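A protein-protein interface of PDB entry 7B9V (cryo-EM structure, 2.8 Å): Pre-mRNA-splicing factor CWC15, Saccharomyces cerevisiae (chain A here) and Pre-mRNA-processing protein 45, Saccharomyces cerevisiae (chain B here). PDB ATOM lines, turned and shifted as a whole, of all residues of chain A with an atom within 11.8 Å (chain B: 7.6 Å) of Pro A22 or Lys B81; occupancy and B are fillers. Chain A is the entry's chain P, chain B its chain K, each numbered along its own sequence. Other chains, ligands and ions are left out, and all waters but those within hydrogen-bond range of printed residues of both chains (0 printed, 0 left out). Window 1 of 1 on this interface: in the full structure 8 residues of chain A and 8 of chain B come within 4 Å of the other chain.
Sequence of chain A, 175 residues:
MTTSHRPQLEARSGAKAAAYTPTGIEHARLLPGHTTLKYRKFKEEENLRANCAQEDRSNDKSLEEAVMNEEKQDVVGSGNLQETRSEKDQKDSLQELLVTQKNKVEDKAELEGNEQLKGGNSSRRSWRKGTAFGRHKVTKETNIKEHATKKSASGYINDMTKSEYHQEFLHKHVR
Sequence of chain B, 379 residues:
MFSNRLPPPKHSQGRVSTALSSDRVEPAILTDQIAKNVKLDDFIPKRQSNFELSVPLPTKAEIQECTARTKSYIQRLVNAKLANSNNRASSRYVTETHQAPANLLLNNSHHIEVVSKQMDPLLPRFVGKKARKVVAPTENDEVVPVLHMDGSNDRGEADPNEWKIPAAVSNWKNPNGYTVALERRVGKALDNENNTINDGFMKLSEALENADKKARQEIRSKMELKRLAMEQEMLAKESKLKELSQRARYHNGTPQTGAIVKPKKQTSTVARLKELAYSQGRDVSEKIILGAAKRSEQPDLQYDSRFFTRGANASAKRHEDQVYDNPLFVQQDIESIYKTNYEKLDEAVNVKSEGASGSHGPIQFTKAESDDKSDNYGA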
ATOM      1  N   GLY A  14      16.078 -44.409  11.088  1.00  0.00           N
ATOM      2  CA  GLY A  14      16.361 -43.011  11.342  1.00  0.00           C
ATOM      3  C   GLY A  14      17.719 -42.741  11.963  1.00  0.00           C
ATOM      4  O   GLY A  14      18.115 -41.572  12.028  1.00  0.00           O
ATOM      5  N   LYS A  16      20.467 -43.451  10.650  1.00  0.00           N
ATOM      6  CA  LYS A  16      21.347 -43.011   9.577  1.00  0.00           C
ATOM      7  C   LYS A  16      21.284 -41.501   9.405  1.00  0.00           C
ATOM      8  O   LYS A  16      22.320 -40.860   9.189  1.00  0.00           O
ATOM      9  CB  LYS A  16      20.991 -43.723   8.275  1.00  0.00           C
ATOM     10  CG  LYS A  16      21.251 -45.212   8.330  1.00  0.00           C
ATOM     11  CD  LYS A  16      20.998 -45.889   7.000  1.00  0.00           C
ATOM     12  CE  LYS A  16      21.412 -47.349   7.063  1.00  0.00           C
ATOM     13  NZ  LYS A  16      21.340 -48.010   5.734  1.00  0.00           N
ATOM     14  N   ALA A  17      20.067 -40.930   9.430  1.00  0.00           N
ATOM     15  CA  ALA A  17      19.913 -39.484   9.304  1.00  0.00           C
ATOM     16  C   ALA A  17      20.554 -38.739  10.467  1.00  0.00           C
ATOM     17  O   ALA A  17      21.027 -37.611  10.292  1.00  0.00           O
ATOM     18  CB  ALA A  17      18.433 -39.120   9.206  1.00  0.00           C
ATOM     19  N   ALA A  18      20.542 -39.339  11.670  1.00  0.00           N
ATOM     20  CA  ALA A  18      21.147 -38.719  12.848  1.00  0.00           C
ATOM     21  C   ALA A  18      22.667 -38.569  12.746  1.00  0.00           C
ATOM     22  O   ALA A  18      23.255 -37.820  13.532  1.00  0.00           O
ATOM     23  CB  ALA A  18      20.791 -39.523  14.099  1.00  0.00           C
ATOM     24  N   ALA A  19      23.312 -39.265  11.802  1.00  0.00           N
ATOM     25  CA  ALA A  19      24.764 -39.353  11.734  1.00  0.00           C
ATOM     26  C   ALA A  19      25.431 -38.139  11.098  1.00  0.00           C
ATOM     27  O   ALA A  19      26.662 -38.053  11.131  1.00  0.00           O
ATOM     28  CB  ALA A  19      25.175 -40.618  10.975  1.00  0.00           C
ATOM     29  N   TYR A  20      24.672 -37.207  10.521  1.00  0.00           N
ATOM     30  CA  TYR A  20      25.275 -36.019   9.931  1.00  0.00           C
ATOM     31  C   TYR A  20      24.351 -34.821  10.103  1.00  0.00           C
ATOM     32  O   TYR A  20      23.147 -34.961  10.328  1.00  0.00           O
ATOM     33  CB  TYR A  20      25.629 -36.218   8.451  1.00  0.00           C
ATOM     34  CG  TYR A  20      24.863 -37.310   7.744  1.00  0.00           C
ATOM     35  CD1 TYR A  20      23.613 -37.057   7.192  1.00  0.00           C
ATOM     36  CD2 TYR A  20      25.401 -38.587   7.603  1.00  0.00           C
ATOM     37  CE1 TYR A  20      22.910 -38.049   6.536  1.00  0.00           C
ATOM     38  CE2 TYR A  20      24.705 -39.587   6.948  1.00  0.00           C
ATOM     39  CZ  TYR A  20      23.461 -39.311   6.417  1.00  0.00           C
ATOM     40  OH  TYR A  20      22.766 -40.302   5.764  1.00  0.00           O
ATOM     41  N   THR A  21      24.939 -33.636   9.966  1.00  0.00           N
ATOM     42  CA  THR A  21      24.369 -32.397  10.465  1.00  0.00           C
ATOM     43  C   THR A  21      23.374 -31.800   9.455  1.00  0.00           C
ATOM     44  O   THR A  21      23.395 -32.167   8.275  1.00  0.00           O
ATOM     45  CB  THR A  21      25.530 -31.431  10.743  1.00  0.00           C
ATOM     46  OG1 THR A  21      26.317 -31.256   9.548  1.00  0.00           O
ATOM     47  CG2 THR A  21      26.411 -31.944  11.873  1.00  0.00           C
ATOM     48  N   PRO A  22      22.464 -30.906   9.899  1.00  0.00           N
ATOM     49  CA  PRO A  22      21.581 -30.206   8.947  1.00  0.00           C
ATOM     50  C   PRO A  22      22.353 -29.285   8.015  1.00  0.00           C
ATOM     51  O   PRO A  22      23.456 -28.847   8.331  1.00  0.00           O
ATOM     52  CB  PRO A  22      20.614 -29.424   9.845  1.00  0.00           C
ATOM     53  CG  PRO A  22      20.702 -30.075  11.152  1.00  0.00           C
ATOM     54  CD  PRO A  22      22.094 -30.551  11.289  1.00  0.00           C
ATOM     55  N   THR A  23      21.777 -29.023   6.839  1.00  0.00           N
ATOM     56  CA  THR A  23      22.423 -28.217   5.806  1.00  0.00           C
ATOM     57  C   THR A  23      21.694 -26.902   5.518  1.00  0.00           C
ATOM     58  O   THR A  23      21.795 -26.356   4.416  1.00  0.00           O
ATOM     59  CB  THR A  23      22.595 -29.034   4.523  1.00  0.00           C
ATOM     60  OG1 THR A  23      23.266 -28.250   3.526  1.00  0.00           O
ATOM     61  CG2 THR A  23      21.261 -29.551   4.003  1.00  0.00           C
ATOM     62  N   GLY A  24      21.026 -26.343   6.527  1.00  0.00           N
ATOM     63  CA  GLY A  24      20.657 -24.938   6.495  1.00  0.00           C
ATOM     64  C   GLY A  24      19.571 -24.510   5.532  1.00  0.00           C
ATOM     65  O   GLY A  24      19.445 -23.314   5.260  1.00  0.00           O
ATOM     66  N   ILE A  25      18.793 -25.440   4.990  1.00  0.00           N
ATOM     67  CA  ILE A  25      17.684 -25.073   4.116  1.00  0.00           C
ATOM     68  C   ILE A  25      16.534 -24.568   4.981  1.00  0.00           C
ATOM     69  O   ILE A  25      16.101 -25.247   5.919  1.00  0.00           O
ATOM     70  CB  ILE A  25      17.247 -26.272   3.257  1.00  0.00           C
ATOM     71  CG1 ILE A  25      18.357 -26.688   2.286  1.00  0.00           C
ATOM     72  CG2 ILE A  25      15.959 -25.975   2.502  1.00  0.00           C
ATOM     73  CD1 ILE A  25      18.697 -25.639   1.249  1.00  0.00           C
ATOM     74  N   GLU A  26      16.042 -23.369   4.671  1.00  0.00           N
ATOM     75  CA  GLU A  26      14.880 -22.811   5.355  1.00  0.00           C
ATOM     76  C   GLU A  26      13.615 -23.376   4.727  1.00  0.00           C
ATOM     77  O   GLU A  26      13.268 -23.033   3.594  1.00  0.00           O
ATOM     78  CB  GLU A  26      14.879 -21.287   5.267  1.00  0.00           C
ATOM     79  CG  GLU A  26      16.058 -20.590   5.920  1.00  0.00           C
ATOM     80  CD  GLU A  26      16.019 -19.087   5.707  1.00  0.00           C
ATOM     81  OE1 GLU A  26      15.038 -18.450   6.149  1.00  0.00           O
ATOM     82  OE2 GLU A  26      16.962 -18.543   5.094  1.00  0.00           O
ATOM     83  N   HIS A  27      12.923 -24.242   5.459  1.00  0.00           N
ATOM     84  CA  HIS A  27      11.620 -24.731   5.040  1.00  0.00           C
ATOM     85  C   HIS A  27      10.542 -23.787   5.542  1.00  0.00           C
ATOM     86  O   HIS A  27      10.695 -23.180   6.606  1.00  0.00           O
ATOM     87  CB  HIS A  27      11.383 -26.139   5.580  1.00  0.00           C
ATOM     88  CG  HIS A  27      12.381 -27.141   5.095  1.00  0.00           C
ATOM     89  ND1 HIS A  27      12.245 -27.803   3.895  1.00  0.00           N
ATOM     90  CD2 HIS A  27      13.540 -27.579   5.640  1.00  0.00           C
ATOM     91  CE1 HIS A  27      13.274 -28.613   3.723  1.00  0.00           C
ATOM     92  NE2 HIS A  27      14.075 -28.496   4.767  1.00  0.00           N
ATOM     93  N   ALA A  28       9.494 -23.608   4.725  1.00  0.00           N
ATOM     94  CA  ALA A  28       8.411 -22.688   5.075  1.00  0.00           C
ATOM     95  C   ALA A  28       7.676 -23.140   6.331  1.00  0.00           C
ATOM     96  O   ALA A  28       7.272 -22.311   7.155  1.00  0.00           O
ATOM     97  CB  ALA A  28       7.439 -22.558   3.907  1.00  0.00           C
ATOM     98  N   ARG A  29       7.473 -24.453   6.481  1.00  0.00           N
ATOM     99  CA  ARG A  29       6.719 -24.969   7.616  1.00  0.00           C
ATOM    100  C   ARG A  29       7.498 -24.892   8.923  1.00  0.00           C
ATOM    101  O   ARG A  29       6.897 -25.028   9.994  1.00  0.00           O
ATOM    102  CB  ARG A  29       6.285 -26.406   7.334  1.00  0.00           C
ATOM    103  CG  ARG A  29       5.140 -26.475   6.347  1.00  0.00           C
ATOM    104  CD  ARG A  29       4.892 -27.873   5.838  1.00  0.00           C
ATOM    105  NE  ARG A  29       3.679 -27.928   5.031  1.00  0.00           N
ATOM    106  CZ  ARG A  29       3.085 -29.046   4.640  1.00  0.00           C
ATOM    107  NH1 ARG A  29       3.564 -30.234   4.967  1.00  0.00           N
ATOM    108  NH2 ARG A  29       1.982 -28.968   3.902  1.00  0.00           N
ATOM    109  N   LEU A  30       8.811 -24.673   8.860  1.00  0.00           N
ATOM    110  CA  LEU A  30       9.641 -24.493  10.040  1.00  0.00           C
ATOM    111  C   LEU A  30       9.883 -23.029  10.385  1.00  0.00           C
ATOM    112  O   LEU A  30      10.691 -22.754  11.279  1.00  0.00           O
ATOM    113  CB  LEU A  30      10.978 -25.213   9.877  1.00  0.00           C
ATOM    114  CG  LEU A  30      11.030 -26.607  10.505  1.00  0.00           C
ATOM    115  CD1 LEU A  30      12.154 -27.424   9.903  1.00  0.00           C
ATOM    116  CD2 LEU A  30      11.187 -26.503  12.018  1.00  0.00           C
ATOM    117  N   LEU A  31       9.237 -22.081   9.690  1.00  0.00           N
ATOM    118  CA  LEU A  31       9.304 -20.676  10.092  1.00  0.00           C
ATOM    119  C   LEU A  31       8.591 -20.487  11.441  1.00  0.00           C
ATOM    120  O   LEU A  31       7.815 -21.367  11.839  1.00  0.00           O
ATOM    121  CB  LEU A  31       8.682 -19.808   8.994  1.00  0.00           C
ATOM    122  CG  LEU A  31       9.360 -19.711   7.631  1.00  0.00           C
ATOM    123  CD1 LEU A  31       8.446 -18.972   6.663  1.00  0.00           C
ATOM    124  CD2 LEU A  31      10.698 -18.998   7.784  1.00  0.00           C
ATOM    125  N   PRO A  32       8.874 -19.393  12.194  1.00  0.00           N
ATOM    126  CA  PRO A  32       8.206 -19.226  13.501  1.00  0.00           C
ATOM    127  C   PRO A  32       6.692 -19.137  13.395  1.00  0.00           C
ATOM    128  O   PRO A  32       6.139 -18.584  12.442  1.00  0.00           O
ATOM    129  CB  PRO A  32       8.822 -17.939  14.063  1.00  0.00           C
ATOM    130  CG  PRO A  32      10.086 -17.797  13.350  1.00  0.00           C
ATOM    131  CD  PRO A  32       9.864 -18.312  11.990  1.00  0.00           C
ATOM    132  N   GLN B  75      17.644 -26.403  26.183  1.00  0.00           N
ATOM    133  CA  GLN B  75      17.583 -25.035  25.674  1.00  0.00           C
ATOM    134  C   GLN B  75      18.893 -24.640  24.993  1.00  0.00           C
ATOM    135  O   GLN B  75      18.869 -23.855  24.033  1.00  0.00           O
ATOM    136  CB  GLN B  75      17.223 -24.046  26.788  1.00  0.00           C
ATOM    137  CG  GLN B  75      16.829 -22.646  26.270  1.00  0.00           C
ATOM    138  CD  GLN B  75      15.667 -22.653  25.271  1.00  0.00           C
ATOM    139  OE1 GLN B  75      15.651 -21.866  24.324  1.00  0.00           O
ATOM    140  NE2 GLN B  75      14.637 -23.451  25.552  1.00  0.00           N
ATOM    141  N   ARG B  76      20.037 -25.162  25.470  1.00  0.00           N
ATOM    142  CA  ARG B  76      21.299 -24.961  24.749  1.00  0.00           C
ATOM    143  C   ARG B  76      21.242 -25.583  23.358  1.00  0.00           C
ATOM    144  O   ARG B  76      21.765 -25.005  22.393  1.00  0.00           O
ATOM    145  CB  ARG B  76      22.476 -25.538  25.533  1.00  0.00           C
ATOM    146  CG  ARG B  76      22.846 -24.769  26.776  1.00  0.00           C
ATOM    147  CD  ARG B  76      24.341 -24.855  27.045  1.00  0.00           C
ATOM    148  NE  ARG B  76      24.799 -26.225  27.255  1.00  0.00           N
ATOM    149  CZ  ARG B  76      24.668 -26.909  28.386  1.00  0.00           C
ATOM    150  NH1 ARG B  76      24.078 -26.384  29.449  1.00  0.00           N
ATOM    151  NH2 ARG B  76      25.139 -28.150  28.452  1.00  0.00           N
ATOM    152  N   LEU B  77      20.624 -26.769  23.236  1.00  0.00           N
ATOM    153  CA  LEU B  77      20.494 -27.389  21.914  1.00  0.00           C
ATOM    154  C   LEU B  77      19.568 -26.591  20.997  1.00  0.00           C
ATOM    155  O   LEU B  77      19.831 -26.492  19.786  1.00  0.00           O
ATOM    156  CB  LEU B  77      20.000 -28.828  22.027  1.00  0.00           C
ATOM    157  CG  LEU B  77      20.889 -29.850  22.720  1.00  0.00           C
ATOM    158  CD1 LEU B  77      20.186 -31.184  22.677  1.00  0.00           C
ATOM    159  CD2 LEU B  77      22.261 -29.927  22.069  1.00  0.00           C
ATOM    160  N   VAL B  78      18.453 -26.072  21.549  1.00  0.00           N
ATOM    161  CA  VAL B  78      17.535 -25.227  20.778  1.00  0.00           C
ATOM    162  C   VAL B  78      18.257 -23.982  20.284  1.00  0.00           C
ATOM    163  O   VAL B  78      18.118 -23.592  19.115  1.00  0.00           O
ATOM    164  CB  VAL B  78      16.300 -24.846  21.630  1.00  0.00           C
ATOM    165  CG1 VAL B  78      15.428 -23.783  20.951  1.00  0.00           C
ATOM    166  CG2 VAL B  78      15.434 -26.038  21.893  1.00  0.00           C
ATOM    167  N   ASN B  79      19.048 -23.358  21.172  1.00  0.00           N
ATOM    168  CA  ASN B  79      19.817 -22.166  20.824  1.00  0.00           C
ATOM    169  C   ASN B  79      20.829 -22.447  19.723  1.00  0.00           C
ATOM    170  O   ASN B  79      21.025 -21.613  18.833  1.00  0.00           O
ATOM    171  CB  ASN B  79      20.523 -21.612  22.062  1.00  0.00           C
ATOM    172  CG  ASN B  79      19.572 -20.915  23.016  1.00  0.00           C
ATOM    173  OD1 ASN B  79      18.359 -20.939  22.825  1.00  0.00           O
ATOM    174  ND2 ASN B  79      20.121 -20.294  24.056  1.00  0.00           N
ATOM    175  N   ALA B  80      21.499 -23.611  19.788  1.00  0.00           N
ATOM    176  CA  ALA B  80      22.480 -23.958  18.762  1.00  0.00           C
ATOM    177  C   ALA B  80      21.831 -24.169  17.400  1.00  0.00           C
ATOM    178  O   ALA B  80      22.335 -23.649  16.380  1.00  0.00           O
ATOM    179  CB  ALA B  80      23.240 -25.213  19.183  1.00  0.00           C
ATOM    180  N   LYS B  81      20.682 -24.881  17.383  1.00  0.00           N
ATOM    181  CA  LYS B  81      19.948 -25.106  16.137  1.00  0.00           C
ATOM    182  C   LYS B  81      19.471 -23.788  15.543  1.00  0.00           C
ATOM    183  O   LYS B  81      19.556 -23.590  14.324  1.00  0.00           O
ATOM    184  CB  LYS B  81      18.774 -26.059  16.384  1.00  0.00           C
ATOM    185  CG  LYS B  81      17.757 -26.193  15.236  1.00  0.00           C
ATOM    186  CD  LYS B  81      18.319 -26.710  13.924  1.00  0.00           C
ATOM    187  CE  LYS B  81      17.196 -26.858  12.902  1.00  0.00           C
ATOM    188  NZ  LYS B  81      17.655 -27.436  11.611  1.00  0.00           N
ATOM    189  N   LEU B  82      18.913 -22.900  16.388  1.00  0.00           N
ATOM    190  CA  LEU B  82      18.398 -21.630  15.889  1.00  0.00           C
ATOM    191  C   LEU B  82      19.528 -20.756  15.357  1.00  0.00           C
ATOM    192  O   LEU B  82      19.433 -20.222  14.247  1.00  0.00           O
ATOM    193  CB  LEU B  82      17.622 -20.903  16.983  1.00  0.00           C
ATOM    194  CG  LEU B  82      16.258 -21.441  17.409  1.00  0.00           C
ATOM    195  CD1 LEU B  82      15.758 -20.674  18.617  1.00  0.00           C
ATOM    196  CD2 LEU B  82      15.261 -21.351  16.268  1.00  0.00           C
ATOM    197  N   ALA B  83      20.597 -20.584  16.166  1.00  0.00           N
ATOM    198  CA  ALA B  83      21.657 -19.627  15.856  1.00  0.00           C
ATOM    199  C   ALA B  83      22.418 -20.015  14.599  1.00  0.00           C
ATOM    200  O   ALA B  83      22.934 -19.144  13.890  1.00  0.00           O
ATOM    201  CB  ALA B  83      22.614 -19.487  17.039  1.00  0.00           C
ATOM    202  N   ASN B  84      22.481 -21.319  14.302  1.00  0.00           N
ATOM    203  CA  ASN B  84      23.190 -21.769  13.114  1.00  0.00           C
ATOM    204  C   ASN B  84      22.330 -21.806  11.856  1.00  0.00           C
ATOM    205  O   ASN B  84      22.864 -22.077  10.777  1.00  0.00           O
ATOM    206  CB  ASN B  84      23.805 -23.143  13.361  1.00  0.00           C
ATOM    207  CG  ASN B  84      24.943 -23.089  14.357  1.00  0.00           C
ATOM    208  OD1 ASN B  84      25.776 -22.185  14.312  1.00  0.00           O
ATOM    209  ND2 ASN B  84      24.973 -24.045  15.276  1.00  0.00           N
ATOM    210  N   SER B  85      21.032 -21.543  11.958  1.00  0.00           N
ATOM    211  CA  SER B  85      20.193 -21.455  10.773  1.00  0.00           C
ATOM    212  C   SER B  85      20.466 -20.166  10.001  1.00  0.00           C
ATOM    213  O   SER B  85      20.975 -19.176  10.534  1.00  0.00           O
ATOM    214  CB  SER B  85      18.720 -21.565  11.133  1.00  0.00           C
ATOM    215  OG  SER B  85      18.318 -20.417  11.812  1.00  0.00           O
ATOM    216  N   ASN B  86      20.102 -20.190   8.723  1.00  0.00           N
ATOM    217  CA  ASN B  86      20.341 -19.065   7.833  1.00  0.00           C
ATOM    218  C   ASN B  86      19.297 -17.962   7.948  1.00  0.00           C
ATOM    219  O   ASN B  86      19.511 -16.885   7.380  1.00  0.00           O
ATOM    220  CB  ASN B  86      20.389 -19.570   6.394  1.00  0.00           C
ATOM    221  CG  ASN B  86      21.686 -20.266   6.073  1.00  0.00           C
ATOM    222  OD1 ASN B  86      22.764 -19.741   6.341  1.00  0.00           O
ATOM    223  ND2 ASN B  86      21.592 -21.466   5.513  1.00  0.00           N
ATOM    224  N   SER B  90      16.078 -15.877  13.208  1.00  0.00           N
ATOM    225  CA  SER B  90      16.211 -16.964  14.175  1.00  0.00           C
ATOM    226  C   SER B  90      16.782 -16.503  15.512  1.00  0.00           C
ATOM    227  O   SER B  90      16.454 -17.084  16.554  1.00  0.00           O
ATOM    228  CB  SER B  90      17.068 -18.073  13.613  1.00  0.00           C
ATOM    229  OG  SER B  90      18.371 -17.618  13.297  1.00  0.00           O
ATOM    230  N   VAL B  94      16.274 -17.092  20.034  1.00  0.00           N
ATOM    231  CA  VAL B  94      17.348 -17.667  20.836  1.00  0.00           C
ATOM    232  C   VAL B  94      17.195 -17.159  22.265  1.00  0.00           C
ATOM    233  O   VAL B  94      17.179 -15.944  22.499  1.00  0.00           O
ATOM    234  CB  VAL B  94      18.722 -17.309  20.255  1.00  0.00           C
ATOM    235  CG1 VAL B  94      19.828 -17.724  21.208  1.00  0.00           C
ATOM    236  CG2 VAL B  94      18.909 -17.963  18.904  1.00  0.00           C
ATOM    237  N   LYS B 129      31.410 -26.531   5.348  1.00  0.00           N
ATOM    238  CA  LYS B 129      30.157 -27.262   5.474  1.00  0.00           C
ATOM    239  C   LYS B 129      29.680 -27.763   4.120  1.00  0.00           C
ATOM    240  O   LYS B 129      29.596 -26.994   3.159  1.00  0.00           O
ATOM    241  CB  LYS B 129      29.099 -26.362   6.100  1.00  0.00           C
ATOM    242  CG  LYS B 129      27.790 -27.006   6.454  1.00  0.00           C
ATOM    243  CD  LYS B 129      26.977 -25.996   7.235  1.00  0.00           C
ATOM    244  CE  LYS B 129      25.678 -26.595   7.684  1.00  0.00           C
ATOM    245  NZ  LYS B 129      25.015 -25.870   8.800  1.00  0.00           N
ATOM    246  N   LYS B 130      29.302 -29.036   4.075  1.00  0.00           N
ATOM    247  CA  LYS B 130      28.741 -29.646   2.878  1.00  0.00           C
ATOM    248  C   LYS B 130      27.804 -30.761   3.295  1.00  0.00           C
ATOM    249  O   LYS B 130      27.852 -31.260   4.420  1.00  0.00           O
ATOM    250  CB  LYS B 130      29.820 -30.221   1.943  1.00  0.00           C
ATOM    251  CG  LYS B 130      30.416 -29.241   0.944  1.00  0.00           C
ATOM    252  CD  LYS B 130      31.463 -29.893   0.058  1.00  0.00           C
ATOM    253  CE  LYS B 130      30.847 -30.907  -0.888  1.00  0.00           C
ATOM    254  NZ  LYS B 130      31.849 -31.392  -1.873  1.00  0.00           N
ATOM    255  N   ALA B 131      26.938 -31.133   2.368  1.00  0.00           N
ATOM    256  CA  ALA B 131      26.140 -32.348   2.472  1.00  0.00           C
ATOM    257  C   ALA B 131      26.991 -33.543   2.060  1.00  0.00           C
ATOM    258  O   ALA B 131      27.265 -33.746   0.875  1.00  0.00           O
ATOM    259  CB  ALA B 131      24.891 -32.215   1.611  1.00  0.00           C
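Printed residues of chain A that touch a printed residue of chain B: Pro A22, Gly A24 and Glu A26. Hydrophobic or aromatic side chains of chain A that line the printed part of chain B: Pro A22. Of the 17 printed residues of chain B, 3 touch a printed residue of chain A. Printed residues of chain B that touch a printed residue of chain A: Lys B81, Asn B86 and Lys B129.
Of chain B, only Lys B81 and Lys B129 come within 4 Å of Pro A22. Of chain A, only Pro A22 (3.98 Å) comes within 4 Å of Lys B81. No residue of chain A comes within 4 Å of Val B78. Ala B80 touches none of the printed residues of chain A. No residue of chain A comes within 4 Å of Leu B82. Of the printed residues of chain B, Glu A26 touches Asn B86. Of the printed residues of chain B, Gly A24 touches Asn B86 (2.8 Å). Of the printed residues of chain A, Asn B86 touches Gly A24 and Glu A26. Leu B77 touches none of the printed residues of chain A. The nearest residue of chain B that does not touch Pro A22 is Lys B130 (6.4 Å). The nearest printed residue of chain A that does not touch Lys B129 is Thr A23 (4.1 Å).
ND2 of Asn B86 is in hydrogen-bond range of O of Gly A24. The backbone carbonyl oxygen (O) of Pro A22 lies close to the side-chain amino group (NZ) of Lys B129 (3.4 Å).
Lys B81 touches Pro A22 (NZ to CB, 3.98 Å). C of Asn B86 touches OE2 of Glu A26 (3.7 Å).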
